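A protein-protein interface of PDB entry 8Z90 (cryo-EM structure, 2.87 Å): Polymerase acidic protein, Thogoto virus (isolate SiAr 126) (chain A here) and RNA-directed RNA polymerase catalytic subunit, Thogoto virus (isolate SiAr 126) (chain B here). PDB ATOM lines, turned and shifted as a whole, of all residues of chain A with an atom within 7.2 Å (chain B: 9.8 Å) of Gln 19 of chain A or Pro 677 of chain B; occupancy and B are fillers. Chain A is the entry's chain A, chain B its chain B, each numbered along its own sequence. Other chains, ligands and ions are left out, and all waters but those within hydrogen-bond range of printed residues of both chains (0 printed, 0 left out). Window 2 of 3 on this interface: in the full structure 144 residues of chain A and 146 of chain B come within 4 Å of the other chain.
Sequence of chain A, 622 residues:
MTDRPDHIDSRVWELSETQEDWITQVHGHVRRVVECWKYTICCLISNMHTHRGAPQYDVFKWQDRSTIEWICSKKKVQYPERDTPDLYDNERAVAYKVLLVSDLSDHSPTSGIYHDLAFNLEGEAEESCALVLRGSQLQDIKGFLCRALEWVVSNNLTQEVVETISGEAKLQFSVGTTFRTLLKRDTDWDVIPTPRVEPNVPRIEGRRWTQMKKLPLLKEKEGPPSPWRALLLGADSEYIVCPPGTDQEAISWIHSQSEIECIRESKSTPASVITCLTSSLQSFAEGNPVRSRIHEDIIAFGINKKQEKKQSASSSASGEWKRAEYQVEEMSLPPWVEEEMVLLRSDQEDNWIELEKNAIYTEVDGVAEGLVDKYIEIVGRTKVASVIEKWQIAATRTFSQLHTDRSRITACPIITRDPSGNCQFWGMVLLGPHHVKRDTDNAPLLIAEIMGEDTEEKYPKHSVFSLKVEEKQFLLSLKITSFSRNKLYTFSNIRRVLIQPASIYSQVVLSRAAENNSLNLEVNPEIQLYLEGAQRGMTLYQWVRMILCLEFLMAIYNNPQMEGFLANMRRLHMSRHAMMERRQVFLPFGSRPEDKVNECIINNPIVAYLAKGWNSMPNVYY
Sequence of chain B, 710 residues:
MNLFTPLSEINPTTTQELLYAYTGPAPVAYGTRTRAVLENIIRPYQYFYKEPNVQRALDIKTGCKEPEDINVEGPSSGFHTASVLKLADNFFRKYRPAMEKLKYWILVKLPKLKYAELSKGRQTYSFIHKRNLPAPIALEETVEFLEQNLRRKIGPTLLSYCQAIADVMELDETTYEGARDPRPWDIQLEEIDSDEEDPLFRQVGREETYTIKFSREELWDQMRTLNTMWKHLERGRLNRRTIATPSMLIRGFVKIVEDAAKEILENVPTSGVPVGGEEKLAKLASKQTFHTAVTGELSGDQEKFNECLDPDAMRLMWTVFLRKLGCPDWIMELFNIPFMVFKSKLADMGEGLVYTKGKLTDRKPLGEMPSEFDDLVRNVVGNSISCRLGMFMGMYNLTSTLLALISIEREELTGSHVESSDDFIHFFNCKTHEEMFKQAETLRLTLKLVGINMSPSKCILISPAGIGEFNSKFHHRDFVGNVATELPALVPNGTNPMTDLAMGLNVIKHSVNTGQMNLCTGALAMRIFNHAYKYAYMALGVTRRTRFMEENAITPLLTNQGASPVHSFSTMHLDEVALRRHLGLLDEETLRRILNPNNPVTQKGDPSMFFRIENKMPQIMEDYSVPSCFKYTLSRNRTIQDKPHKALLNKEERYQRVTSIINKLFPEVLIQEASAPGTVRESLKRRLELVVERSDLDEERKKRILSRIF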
ATOM      1  N   VAL A  12      16.579 -30.261 -19.162  1.00  0.00           N
ATOM      2  CA  VAL A  12      16.339 -29.682 -17.845  1.00  0.00           C
ATOM      3  C   VAL A  12      17.555 -29.874 -16.949  1.00  0.00           C
ATOM      4  O   VAL A  12      17.875 -29.011 -16.126  1.00  0.00           O
ATOM      5  CB  VAL A  12      15.063 -30.275 -17.217  1.00  0.00           C
ATOM      6  CG1 VAL A  12      13.832 -29.732 -17.918  1.00  0.00           C
ATOM      7  CG2 VAL A  12      15.081 -31.783 -17.278  1.00  0.00           C
ATOM      8  N   GLU A  14      20.770 -29.948 -17.933  1.00  0.00           N
ATOM      9  CA  GLU A  14      21.767 -28.962 -18.336  1.00  0.00           C
ATOM     10  C   GLU A  14      21.362 -27.561 -17.900  1.00  0.00           C
ATOM     11  O   GLU A  14      22.210 -26.762 -17.486  1.00  0.00           O
ATOM     12  CB  GLU A  14      21.979 -29.014 -19.848  1.00  0.00           C
ATOM     13  CG  GLU A  14      22.599 -30.312 -20.339  1.00  0.00           C
ATOM     14  CD  GLU A  14      24.024 -30.495 -19.856  1.00  0.00           C
ATOM     15  OE1 GLU A  14      24.733 -29.480 -19.686  1.00  0.00           O
ATOM     16  OE2 GLU A  14      24.437 -31.654 -19.643  1.00  0.00           O
ATOM     17  N   LEU A  15      20.069 -27.241 -17.990  1.00  0.00           N
ATOM     18  CA  LEU A  15      19.597 -25.947 -17.515  1.00  0.00           C
ATOM     19  C   LEU A  15      19.759 -25.798 -16.007  1.00  0.00           C
ATOM     20  O   LEU A  15      20.065 -24.699 -15.535  1.00  0.00           O
ATOM     21  CB  LEU A  15      18.133 -25.753 -17.918  1.00  0.00           C
ATOM     22  CG  LEU A  15      17.360 -24.582 -17.313  1.00  0.00           C
ATOM     23  CD1 LEU A  15      17.891 -23.266 -17.853  1.00  0.00           C
ATOM     24  CD2 LEU A  15      15.878 -24.719 -17.604  1.00  0.00           C
ATOM     25  N   SER A  16      19.575 -26.882 -15.250  1.00  0.00           N
ATOM     26  CA  SER A  16      19.691 -26.839 -13.797  1.00  0.00           C
ATOM     27  C   SER A  16      21.142 -26.775 -13.340  1.00  0.00           C
ATOM     28  O   SER A  16      21.419 -26.312 -12.228  1.00  0.00           O
ATOM     29  CB  SER A  16      19.013 -28.063 -13.186  1.00  0.00           C
ATOM     30  OG  SER A  16      19.769 -29.235 -13.428  1.00  0.00           O
ATOM     31  N   GLU A  17      22.066 -27.260 -14.173  1.00  0.00           N
ATOM     32  CA  GLU A  17      23.484 -27.347 -13.826  1.00  0.00           C
ATOM     33  C   GLU A  17      24.035 -26.128 -13.090  1.00  0.00           C
ATOM     34  O   GLU A  17      24.864 -26.275 -12.188  1.00  0.00           O
ATOM     35  CB  GLU A  17      24.313 -27.584 -15.093  1.00  0.00           C
ATOM     36  CG  GLU A  17      25.812 -27.732 -14.851  1.00  0.00           C
ATOM     37  CD  GLU A  17      26.170 -28.963 -14.041  1.00  0.00           C
ATOM     38  OE1 GLU A  17      25.398 -29.943 -14.067  1.00  0.00           O
ATOM     39  OE2 GLU A  17      27.225 -28.948 -13.374  1.00  0.00           O
ATOM     40  N   THR A  18      23.585 -24.925 -13.449  1.00  0.00           N
ATOM     41  CA  THR A  18      24.178 -23.706 -12.912  1.00  0.00           C
ATOM     42  C   THR A  18      23.168 -22.744 -12.296  1.00  0.00           C
ATOM     43  O   THR A  18      23.504 -21.574 -12.081  1.00  0.00           O
ATOM     44  CB  THR A  18      24.976 -22.988 -14.003  1.00  0.00           C
ATOM     45  OG1 THR A  18      24.219 -22.973 -15.219  1.00  0.00           O
ATOM     46  CG2 THR A  18      26.295 -23.705 -14.242  1.00  0.00           C
ATOM     47  N   GLN A  19      21.945 -23.192 -12.004  1.00  0.00           N
ATOM     48  CA  GLN A  19      20.982 -22.301 -11.365  1.00  0.00           C
ATOM     49  C   GLN A  19      21.330 -22.027  -9.909  1.00  0.00           C
ATOM     50  O   GLN A  19      21.248 -20.879  -9.461  1.00  0.00           O
ATOM     51  CB  GLN A  19      19.572 -22.881 -11.468  1.00  0.00           C
ATOM     52  CG  GLN A  19      19.180 -23.252 -12.879  1.00  0.00           C
ATOM     53  CD  GLN A  19      18.998 -22.036 -13.762  1.00  0.00           C
ATOM     54  OE1 GLN A  19      18.696 -20.943 -13.282  1.00  0.00           O
ATOM     55  NE2 GLN A  19      19.196 -22.215 -15.061  1.00  0.00           N
ATOM     56  N   GLU A  20      21.715 -23.057  -9.161  1.00  0.00           N
ATOM     57  CA  GLU A  20      22.181 -22.886  -7.794  1.00  0.00           C
ATOM     58  C   GLU A  20      23.448 -23.708  -7.623  1.00  0.00           C
ATOM     59  O   GLU A  20      23.725 -24.630  -8.395  1.00  0.00           O
ATOM     60  CB  GLU A  20      21.114 -23.298  -6.775  1.00  0.00           C
ATOM     61  CG  GLU A  20      19.893 -22.391  -6.742  1.00  0.00           C
ATOM     62  CD  GLU A  20      18.620 -23.139  -6.397  1.00  0.00           C
ATOM     63  OE1 GLU A  20      18.597 -23.829  -5.357  1.00  0.00           O
ATOM     64  OE2 GLU A  20      17.642 -23.037  -7.167  1.00  0.00           O
ATOM     65  N   ASP A  21      24.222 -23.363  -6.595  1.00  0.00           N
ATOM     66  CA  ASP A  21      25.504 -24.015  -6.344  1.00  0.00           C
ATOM     67  C   ASP A  21      25.256 -25.292  -5.548  1.00  0.00           C
ATOM     68  O   ASP A  21      25.319 -25.327  -4.318  1.00  0.00           O
ATOM     69  CB  ASP A  21      26.452 -23.071  -5.621  1.00  0.00           C
ATOM     70  CG  ASP A  21      27.831 -23.653  -5.469  1.00  0.00           C
ATOM     71  OD1 ASP A  21      28.564 -23.703  -6.478  1.00  0.00           O
ATOM     72  OD2 ASP A  21      28.188 -24.064  -4.348  1.00  0.00           O
ATOM     73  N   TRP A  22      24.972 -26.368  -6.285  1.00  0.00           N
ATOM     74  CA  TRP A  22      24.593 -27.635  -5.666  1.00  0.00           C
ATOM     75  C   TRP A  22      25.727 -28.221  -4.832  1.00  0.00           C
ATOM     76  O   TRP A  22      25.498 -28.766  -3.747  1.00  0.00           O
ATOM     77  CB  TRP A  22      24.158 -28.625  -6.746  1.00  0.00           C
ATOM     78  CG  TRP A  22      23.208 -28.050  -7.753  1.00  0.00           C
ATOM     79  CD1 TRP A  22      23.390 -27.983  -9.101  1.00  0.00           C
ATOM     80  CD2 TRP A  22      21.919 -27.477  -7.494  1.00  0.00           C
ATOM     81  NE1 TRP A  22      22.303 -27.396  -9.700  1.00  0.00           N
ATOM     82  CE2 TRP A  22      21.385 -27.077  -8.735  1.00  0.00           C
ATOM     83  CE3 TRP A  22      21.167 -27.262  -6.336  1.00  0.00           C
ATOM     84  CZ2 TRP A  22      20.135 -26.473  -8.849  1.00  0.00           C
ATOM     85  CZ3 TRP A  22      19.926 -26.662  -6.453  1.00  0.00           C
ATOM     86  CH2 TRP A  22      19.423 -26.275  -7.699  1.00  0.00           C
ATOM     87  N   GLU A  35      14.443 -29.732  -7.685  1.00  0.00           N
ATOM     88  CA  GLU A  35      14.195 -28.577  -8.541  1.00  0.00           C
ATOM     89  C   GLU A  35      13.919 -28.987  -9.982  1.00  0.00           C
ATOM     90  O   GLU A  35      13.077 -28.371 -10.648  1.00  0.00           O
ATOM     91  CB  GLU A  35      15.374 -27.607  -8.479  1.00  0.00           C
ATOM     92  CG  GLU A  35      15.694 -27.106  -7.082  1.00  0.00           C
ATOM     93  CD  GLU A  35      14.700 -26.073  -6.591  1.00  0.00           C
ATOM     94  OE1 GLU A  35      13.951 -25.521  -7.423  1.00  0.00           O
ATOM     95  OE2 GLU A  35      14.667 -25.813  -5.368  1.00  0.00           O
ATOM     96  N   LYS A  61      10.297 -19.923 -14.277  1.00  0.00           N
ATOM     97  CA  LYS A  61      11.347 -20.577 -13.511  1.00  0.00           C
ATOM     98  C   LYS A  61      12.533 -20.869 -14.419  1.00  0.00           C
ATOM     99  O   LYS A  61      12.352 -21.310 -15.558  1.00  0.00           O
ATOM    100  CB  LYS A  61      10.833 -21.872 -12.880  1.00  0.00           C
ATOM    101  CG  LYS A  61      11.828 -22.558 -11.957  1.00  0.00           C
ATOM    102  CD  LYS A  61      11.473 -24.023 -11.755  1.00  0.00           C
ATOM    103  CE  LYS A  61      11.669 -24.449 -10.311  1.00  0.00           C
ATOM    104  NZ  LYS A  61      13.101 -24.409  -9.907  1.00  0.00           N
ATOM    105  N   TRP A  62      13.740 -20.613 -13.910  1.00  0.00           N
ATOM    106  CA  TRP A  62      14.981 -20.932 -14.618  1.00  0.00           C
ATOM    107  C   TRP A  62      15.058 -20.208 -15.960  1.00  0.00           C
ATOM    108  O   TRP A  62      15.512 -20.763 -16.963  1.00  0.00           O
ATOM    109  CB  TRP A  62      15.128 -22.442 -14.799  1.00  0.00           C
ATOM    110  CG  TRP A  62      15.459 -23.148 -13.530  1.00  0.00           C
ATOM    111  CD1 TRP A  62      15.672 -22.580 -12.309  1.00  0.00           C
ATOM    112  CD2 TRP A  62      15.565 -24.562 -13.338  1.00  0.00           C
ATOM    113  NE1 TRP A  62      15.933 -23.551 -11.374  1.00  0.00           N
ATOM    114  CE2 TRP A  62      15.870 -24.777 -11.981  1.00  0.00           C
ATOM    115  CE3 TRP A  62      15.443 -25.667 -14.185  1.00  0.00           C
ATOM    116  CZ2 TRP A  62      16.054 -26.048 -11.452  1.00  0.00           C
ATOM    117  CZ3 TRP A  62      15.626 -26.928 -13.656  1.00  0.00           C
ATOM    118  CH2 TRP A  62      15.923 -27.109 -12.302  1.00  0.00           C
ATOM    119  N   GLN A  63      14.608 -18.957 -15.977  1.00  0.00           N
ATOM    120  CA  GLN A  63      14.627 -18.123 -17.169  1.00  0.00           C
ATOM    121  C   GLN A  63      15.350 -16.825 -16.843  1.00  0.00           C
ATOM    122  O   GLN A  63      15.385 -16.403 -15.683  1.00  0.00           O
ATOM    123  CB  GLN A  63      13.198 -17.842 -17.667  1.00  0.00           C
ATOM    124  CG  GLN A  63      13.112 -16.977 -18.915  1.00  0.00           C
ATOM    125  CD  GLN A  63      11.772 -17.087 -19.611  1.00  0.00           C
ATOM    126  OE1 GLN A  63      10.743 -16.682 -19.072  1.00  0.00           O
ATOM    127  NE2 GLN A  63      11.777 -17.636 -20.821  1.00  0.00           N
ATOM    128  N   ASP A  64      15.943 -16.209 -17.865  1.00  0.00           N
ATOM    129  CA  ASP A  64      16.656 -14.951 -17.683  1.00  0.00           C
ATOM    130  C   ASP A  64      15.740 -13.905 -17.059  1.00  0.00           C
ATOM    131  O   ASP A  64      14.583 -13.756 -17.458  1.00  0.00           O
ATOM    132  CB  ASP A  64      17.193 -14.454 -19.026  1.00  0.00           C
ATOM    133  CG  ASP A  64      17.901 -13.120 -18.914  1.00  0.00           C
ATOM    134  OD1 ASP A  64      18.732 -12.961 -17.995  1.00  0.00           O
ATOM    135  OD2 ASP A  64      17.628 -12.230 -19.746  1.00  0.00           O
ATOM    136  N   ARG A  65      16.272 -13.186 -16.068  1.00  0.00           N
ATOM    137  CA  ARG A  65      15.447 -12.272 -15.284  1.00  0.00           C
ATOM    138  C   ARG A  65      14.903 -11.131 -16.138  1.00  0.00           C
ATOM    139  O   ARG A  65      13.753 -10.714 -15.966  1.00  0.00           O
ATOM    140  CB  ARG A  65      16.252 -11.727 -14.103  1.00  0.00           C
ATOM    141  CG  ARG A  65      15.643 -10.504 -13.435  1.00  0.00           C
ATOM    142  CD  ARG A  65      14.304 -10.830 -12.787  1.00  0.00           C
ATOM    143  NE  ARG A  65      14.308 -12.132 -12.133  1.00  0.00           N
ATOM    144  CZ  ARG A  65      13.360 -12.558 -11.310  1.00  0.00           C
ATOM    145  NH1 ARG A  65      12.311 -11.809 -11.018  1.00  0.00           N
ATOM    146  NH2 ARG A  65      13.468 -13.768 -10.769  1.00  0.00           N
ATOM    147  N   LYS B 153      30.588 -27.915 -13.599  1.00  0.00           N
ATOM    148  CA  LYS B 153      30.743 -26.473 -13.744  1.00  0.00           C
ATOM    149  C   LYS B 153      30.984 -25.855 -12.373  1.00  0.00           C
ATOM    150  O   LYS B 153      30.186 -26.049 -11.451  1.00  0.00           O
ATOM    151  CB  LYS B 153      29.512 -25.856 -14.406  1.00  0.00           C
ATOM    152  CG  LYS B 153      29.230 -26.389 -15.799  1.00  0.00           C
ATOM    153  CD  LYS B 153      30.338 -26.014 -16.767  1.00  0.00           C
ATOM    154  CE  LYS B 153      29.855 -26.072 -18.205  1.00  0.00           C
ATOM    155  NZ  LYS B 153      29.078 -27.312 -18.476  1.00  0.00           N
ATOM    156  N   ILE B 154      32.085 -25.114 -12.244  1.00  0.00           N
ATOM    157  CA  ILE B 154      32.410 -24.473 -10.977  1.00  0.00           C
ATOM    158  C   ILE B 154      31.494 -23.275 -10.759  1.00  0.00           C
ATOM    159  O   ILE B 154      31.272 -22.456 -11.661  1.00  0.00           O
ATOM    160  CB  ILE B 154      33.891 -24.052 -10.938  1.00  0.00           C
ATOM    161  CG1 ILE B 154      34.792 -25.178 -11.450  1.00  0.00           C
ATOM    162  CG2 ILE B 154      34.294 -23.650  -9.530  1.00  0.00           C
ATOM    163  CD1 ILE B 154      34.552 -26.521 -10.791  1.00  0.00           C
ATOM    164  N   GLY B 155      30.955 -23.169  -9.548  1.00  0.00           N
ATOM    165  CA  GLY B 155      30.072 -22.082  -9.205  1.00  0.00           C
ATOM    166  C   GLY B 155      30.805 -20.760  -9.127  1.00  0.00           C
ATOM    167  O   GLY B 155      32.030 -20.710  -8.980  1.00  0.00           O
ATOM    168  N   PRO B 156      30.063 -19.655  -9.231  1.00  0.00           N
ATOM    169  CA  PRO B 156      30.708 -18.334  -9.229  1.00  0.00           C
ATOM    170  C   PRO B 156      31.386 -17.975  -7.918  1.00  0.00           C
ATOM    171  O   PRO B 156      32.260 -17.101  -7.919  1.00  0.00           O
ATOM    172  CB  PRO B 156      29.546 -17.383  -9.535  1.00  0.00           C
ATOM    173  CG  PRO B 156      28.357 -18.084  -8.972  1.00  0.00           C
ATOM    174  CD  PRO B 156      28.593 -19.547  -9.258  1.00  0.00           C
ATOM    175  N   PHE B 666      24.908  -6.190 -22.777  1.00  0.00           N
ATOM    176  CA  PHE B 666      24.730  -6.160 -21.333  1.00  0.00           C
ATOM    177  C   PHE B 666      25.337  -4.880 -20.772  1.00  0.00           C
ATOM    178  O   PHE B 666      26.528  -4.853 -20.440  1.00  0.00           O
ATOM    179  CB  PHE B 666      25.383  -7.379 -20.680  1.00  0.00           C
ATOM    180  CG  PHE B 666      24.707  -8.680 -21.005  1.00  0.00           C
ATOM    181  CD1 PHE B 666      25.008  -9.361 -22.170  1.00  0.00           C
ATOM    182  CD2 PHE B 666      23.783  -9.230 -20.136  1.00  0.00           C
ATOM    183  CE1 PHE B 666      24.391 -10.557 -22.468  1.00  0.00           C
ATOM    184  CE2 PHE B 666      23.164 -10.428 -20.430  1.00  0.00           C
ATOM    185  CZ  PHE B 666      23.468 -11.091 -21.597  1.00  0.00           C
ATOM    186  N   GLU B 673      28.583  -6.660 -10.932  1.00  0.00           N
ATOM    187  CA  GLU B 673      29.174  -7.877 -11.461  1.00  0.00           C
ATOM    188  C   GLU B 673      28.136  -8.677 -12.244  1.00  0.00           C
ATOM    189  O   GLU B 673      26.926  -8.456 -12.142  1.00  0.00           O
ATOM    190  CB  GLU B 673      29.755  -8.726 -10.330  1.00  0.00           C
ATOM    191  CG  GLU B 673      30.954  -8.104  -9.629  1.00  0.00           C
ATOM    192  CD  GLU B 673      30.556  -7.099  -8.564  1.00  0.00           C
ATOM    193  OE1 GLU B 673      29.342  -6.929  -8.326  1.00  0.00           O
ATOM    194  OE2 GLU B 673      31.458  -6.478  -7.965  1.00  0.00           O
ATOM    195  N   ALA B 674      28.627  -9.622 -13.041  1.00  0.00           N
ATOM    196  CA  ALA B 674      27.752 -10.494 -13.811  1.00  0.00           C
ATOM    197  C   ALA B 674      27.259 -11.636 -12.932  1.00  0.00           C
ATOM    198  O   ALA B 674      28.058 -12.348 -12.318  1.00  0.00           O
ATOM    199  CB  ALA B 674      28.484 -11.042 -15.034  1.00  0.00           C
ATOM    200  N   SER B 675      25.938 -11.809 -12.874  1.00  0.00           N
ATOM    201  CA  SER B 675      25.336 -12.825 -12.025  1.00  0.00           C
ATOM    202  C   SER B 675      24.321 -13.701 -12.746  1.00  0.00           C
ATOM    203  O   SER B 675      23.669 -14.522 -12.093  1.00  0.00           O
ATOM    204  CB  SER B 675      24.660 -12.174 -10.809  1.00  0.00           C
ATOM    205  OG  SER B 675      25.602 -11.894  -9.789  1.00  0.00           O
ATOM    206  N   ALA B 676      24.166 -13.553 -14.055  1.00  0.00           N
ATOM    207  CA  ALA B 676      23.201 -14.365 -14.782  1.00  0.00           C
ATOM    208  C   ALA B 676      23.670 -15.815 -14.824  1.00  0.00           C
ATOM    209  O   ALA B 676      24.799 -16.084 -15.252  1.00  0.00           O
ATOM    210  CB  ALA B 676      23.009 -13.829 -16.198  1.00  0.00           C
ATOM    211  N   PRO B 677      22.847 -16.771 -14.393  1.00  0.00           N
ATOM    212  CA  PRO B 677      23.254 -18.183 -14.421  1.00  0.00           C
ATOM    213  C   PRO B 677      23.091 -18.764 -15.818  1.00  0.00           C
ATOM    214  O   PRO B 677      22.027 -18.658 -16.430  1.00  0.00           O
ATOM    215  CB  PRO B 677      22.303 -18.843 -13.418  1.00  0.00           C
ATOM    216  CG  PRO B 677      21.058 -18.020 -13.514  1.00  0.00           C
ATOM    217  CD  PRO B 677      21.481 -16.604 -13.862  1.00  0.00           C
ATOM    218  N   GLY B 678      24.158 -19.375 -16.326  1.00  0.00           N
ATOM    219  CA  GLY B 678      24.137 -19.958 -17.652  1.00  0.00           C
ATOM    220  C   GLY B 678      25.414 -19.703 -18.423  1.00  0.00           C
ATOM    221  O   GLY B 678      26.352 -19.099 -17.896  1.00  0.00           O
ATOM    222  N   THR B 679      25.464 -20.156 -19.671  1.00  0.00           N
ATOM    223  CA  THR B 679      26.643 -19.968 -20.502  1.00  0.00           C
ATOM    224  C   THR B 679      26.604 -18.581 -21.141  1.00  0.00           C
ATOM    225  O   THR B 679      25.595 -17.872 -21.092  1.00  0.00           O
ATOM    226  CB  THR B 679      26.739 -21.070 -21.552  1.00  0.00           C
ATOM    227  OG1 THR B 679      25.567 -21.053 -22.375  1.00  0.00           O
ATOM    228  CG2 THR B 679      26.863 -22.430 -20.885  1.00  0.00           C
ATOM    229  N   VAL B 680      27.716 -18.178 -21.748  1.00  0.00           N
ATOM    230  CA  VAL B 680      27.801 -16.913 -22.462  1.00  0.00           C
ATOM    231  C   VAL B 680      26.946 -16.925 -23.724  1.00  0.00           C
ATOM    232  O   VAL B 680      26.253 -15.951 -24.015  1.00  0.00           O
ATOM    233  CB  VAL B 680      29.275 -16.588 -22.788  1.00  0.00           C
ATOM    234  CG1 VAL B 680      29.369 -15.410 -23.739  1.00  0.00           C
ATOM    235  CG2 VAL B 680      30.050 -16.310 -21.510  1.00  0.00           C
ATOM    236  N   ARG B 681      26.982 -18.033 -24.471  1.00  0.00           N
ATOM    237  CA  ARG B 681      26.206 -18.129 -25.702  1.00  0.00           C
ATOM    238  C   ARG B 681      24.714 -17.979 -25.435  1.00  0.00           C
ATOM    239  O   ARG B 681      24.026 -17.218 -26.127  1.00  0.00           O
ATOM    240  CB  ARG B 681      26.486 -19.465 -26.390  1.00  0.00           C
ATOM    241  CG  ARG B 681      25.982 -19.550 -27.820  1.00  0.00           C
ATOM    242  CD  ARG B 681      26.342 -20.882 -28.456  1.00  0.00           C
ATOM    243  NE  ARG B 681      27.655 -20.861 -29.093  1.00  0.00           N
ATOM    244  CZ  ARG B 681      28.713 -21.522 -28.647  1.00  0.00           C
ATOM    245  NH1 ARG B 681      28.653 -22.268 -27.557  1.00  0.00           N
ATOM    246  NH2 ARG B 681      29.861 -21.435 -29.314  1.00  0.00           N
ATOM    247  N   GLU B 682      24.196 -18.697 -24.436  1.00  0.00           N
ATOM    248  CA  GLU B 682      22.766 -18.644 -24.149  1.00  0.00           C
ATOM    249  C   GLU B 682      22.340 -17.260 -23.679  1.00  0.00           C
ATOM    250  O   GLU B 682      21.303 -16.744 -24.111  1.00  0.00           O
ATOM    251  CB  GLU B 682      22.402 -19.700 -23.105  1.00  0.00           C
ATOM    252  CG  GLU B 682      22.577 -21.131 -23.584  1.00  0.00           C
ATOM    253  CD  GLU B 682      21.610 -21.499 -24.691  1.00  0.00           C
ATOM    254  OE1 GLU B 682      20.481 -20.965 -24.699  1.00  0.00           O
ATOM    255  OE2 GLU B 682      21.978 -22.324 -25.554  1.00  0.00           O
ATOM    256  N   SER B 683      23.124 -16.647 -22.788  1.00  0.00           N
ATOM    257  CA  SER B 683      22.786 -15.314 -22.301  1.00  0.00           C
ATOM    258  C   SER B 683      22.808 -14.292 -23.430  1.00  0.00           C
ATOM    259  O   SER B 683      21.911 -13.447 -23.529  1.00  0.00           O
ATOM    260  CB  SER B 683      23.746 -14.903 -21.187  1.00  0.00           C
ATOM    261  OG  SER B 683      23.870 -15.929 -20.217  1.00  0.00           O
ATOM    262  N   LEU B 684      23.825 -14.358 -24.292  1.00  0.00           N
ATOM    263  CA  LEU B 684      23.899 -13.432 -25.417  1.00  0.00           C
ATOM    264  C   LEU B 684      22.736 -13.634 -26.380  1.00  0.00           C
ATOM    265  O   LEU B 684      22.159 -12.658 -26.872  1.00  0.00           O
ATOM    266  CB  LEU B 684      25.234 -13.596 -26.138  1.00  0.00           C
ATOM    267  CG  LEU B 684      26.440 -12.996 -25.415  1.00  0.00           C
ATOM    268  CD1 LEU B 684      27.699 -13.268 -26.195  1.00  0.00           C
ATOM    269  CD2 LEU B 684      26.258 -11.505 -25.218  1.00  0.00           C
ATOM    270  N   ARG B 686      19.718 -14.865 -25.670  1.00  0.00           N
ATOM    271  CA  ARG B 686      18.503 -14.375 -25.032  1.00  0.00           C
ATOM    272  C   ARG B 686      18.454 -12.857 -25.012  1.00  0.00           C
ATOM    273  O   ARG B 686      17.385 -12.274 -25.218  1.00  0.00           O
ATOM    274  CB  ARG B 686      18.382 -14.927 -23.611  1.00  0.00           C
ATOM    275  CG  ARG B 686      17.850 -16.353 -23.522  1.00  0.00           C
ATOM    276  CD  ARG B 686      16.501 -16.531 -24.223  1.00  0.00           C
ATOM    277  NE  ARG B 686      15.643 -15.355 -24.121  1.00  0.00           N
ATOM    278  CZ  ARG B 686      14.592 -15.125 -24.898  1.00  0.00           C
ATOM    279  NH1 ARG B 686      14.223 -15.984 -25.831  1.00  0.00           N
ATOM    280  NH2 ARG B 686      13.892 -14.006 -24.730  1.00  0.00           N
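O of Leu 15 of chain A sits at hydrogen-bond distance from NE2 of Gln 19 of chain A (2.7 Å).
N of Lys 153 of chain B touches OE2 of Glu 17 of chain A (3.5 Å).
Lys 153 of chain B touches Thr 18 of chain A.
O of Thr 18 of chain A touches CB of Pro 677 of chain B, at 3.3 Å.
Thr 18 of chain A touches Gly 678 of chain B.
Gln 19 of chain A touches Pro 677 of chain B.
Gly 155 of chain B touches Asp 21 of chain A (CA to OD1, 3.5 Å).
No residue of chain B comes within 4 Å of Glu 20 of chain A.
Trp 62 of chain A touches none of the printed residues of chain B.
Printed residues of chain A within 4 Å of Lys 153 of chain B: Glu 17 (3.5 Å) and Thr 18 (3.9 Å).
Phe 666 of chain B touches none of the printed residues of chain A.
Of chain A, only Thr 18 and Gln 19 come within 4 Å of Pro 677 of chain B.
Of the printed residues of chain A, Gly 678 of chain B touches Thr 18 (3.8 Å).
The nearest residue of chain B that does not touch Gln 19 of chain A is Gly 678 of chain B (5.9 Å).
The nearest residue of chain A that does not touch Pro 677 of chain B is Glu 20 of chain A (6.0 Å).
Of the 16 printed residues of chain A, 4 touch a printed residue of chain B.
Of the 18 printed residues of chain B, 4 touch a printed residue of chain A.
Printed residues of chain B that touch a printed residue of chain A: Lys 153, Gly 155, Pro 677 and Gly 678.
Among the printed residues, no Asp or Glu carboxylate lies within 4 Å of a Lys or Arg side-chain nitrogen of the other chain.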
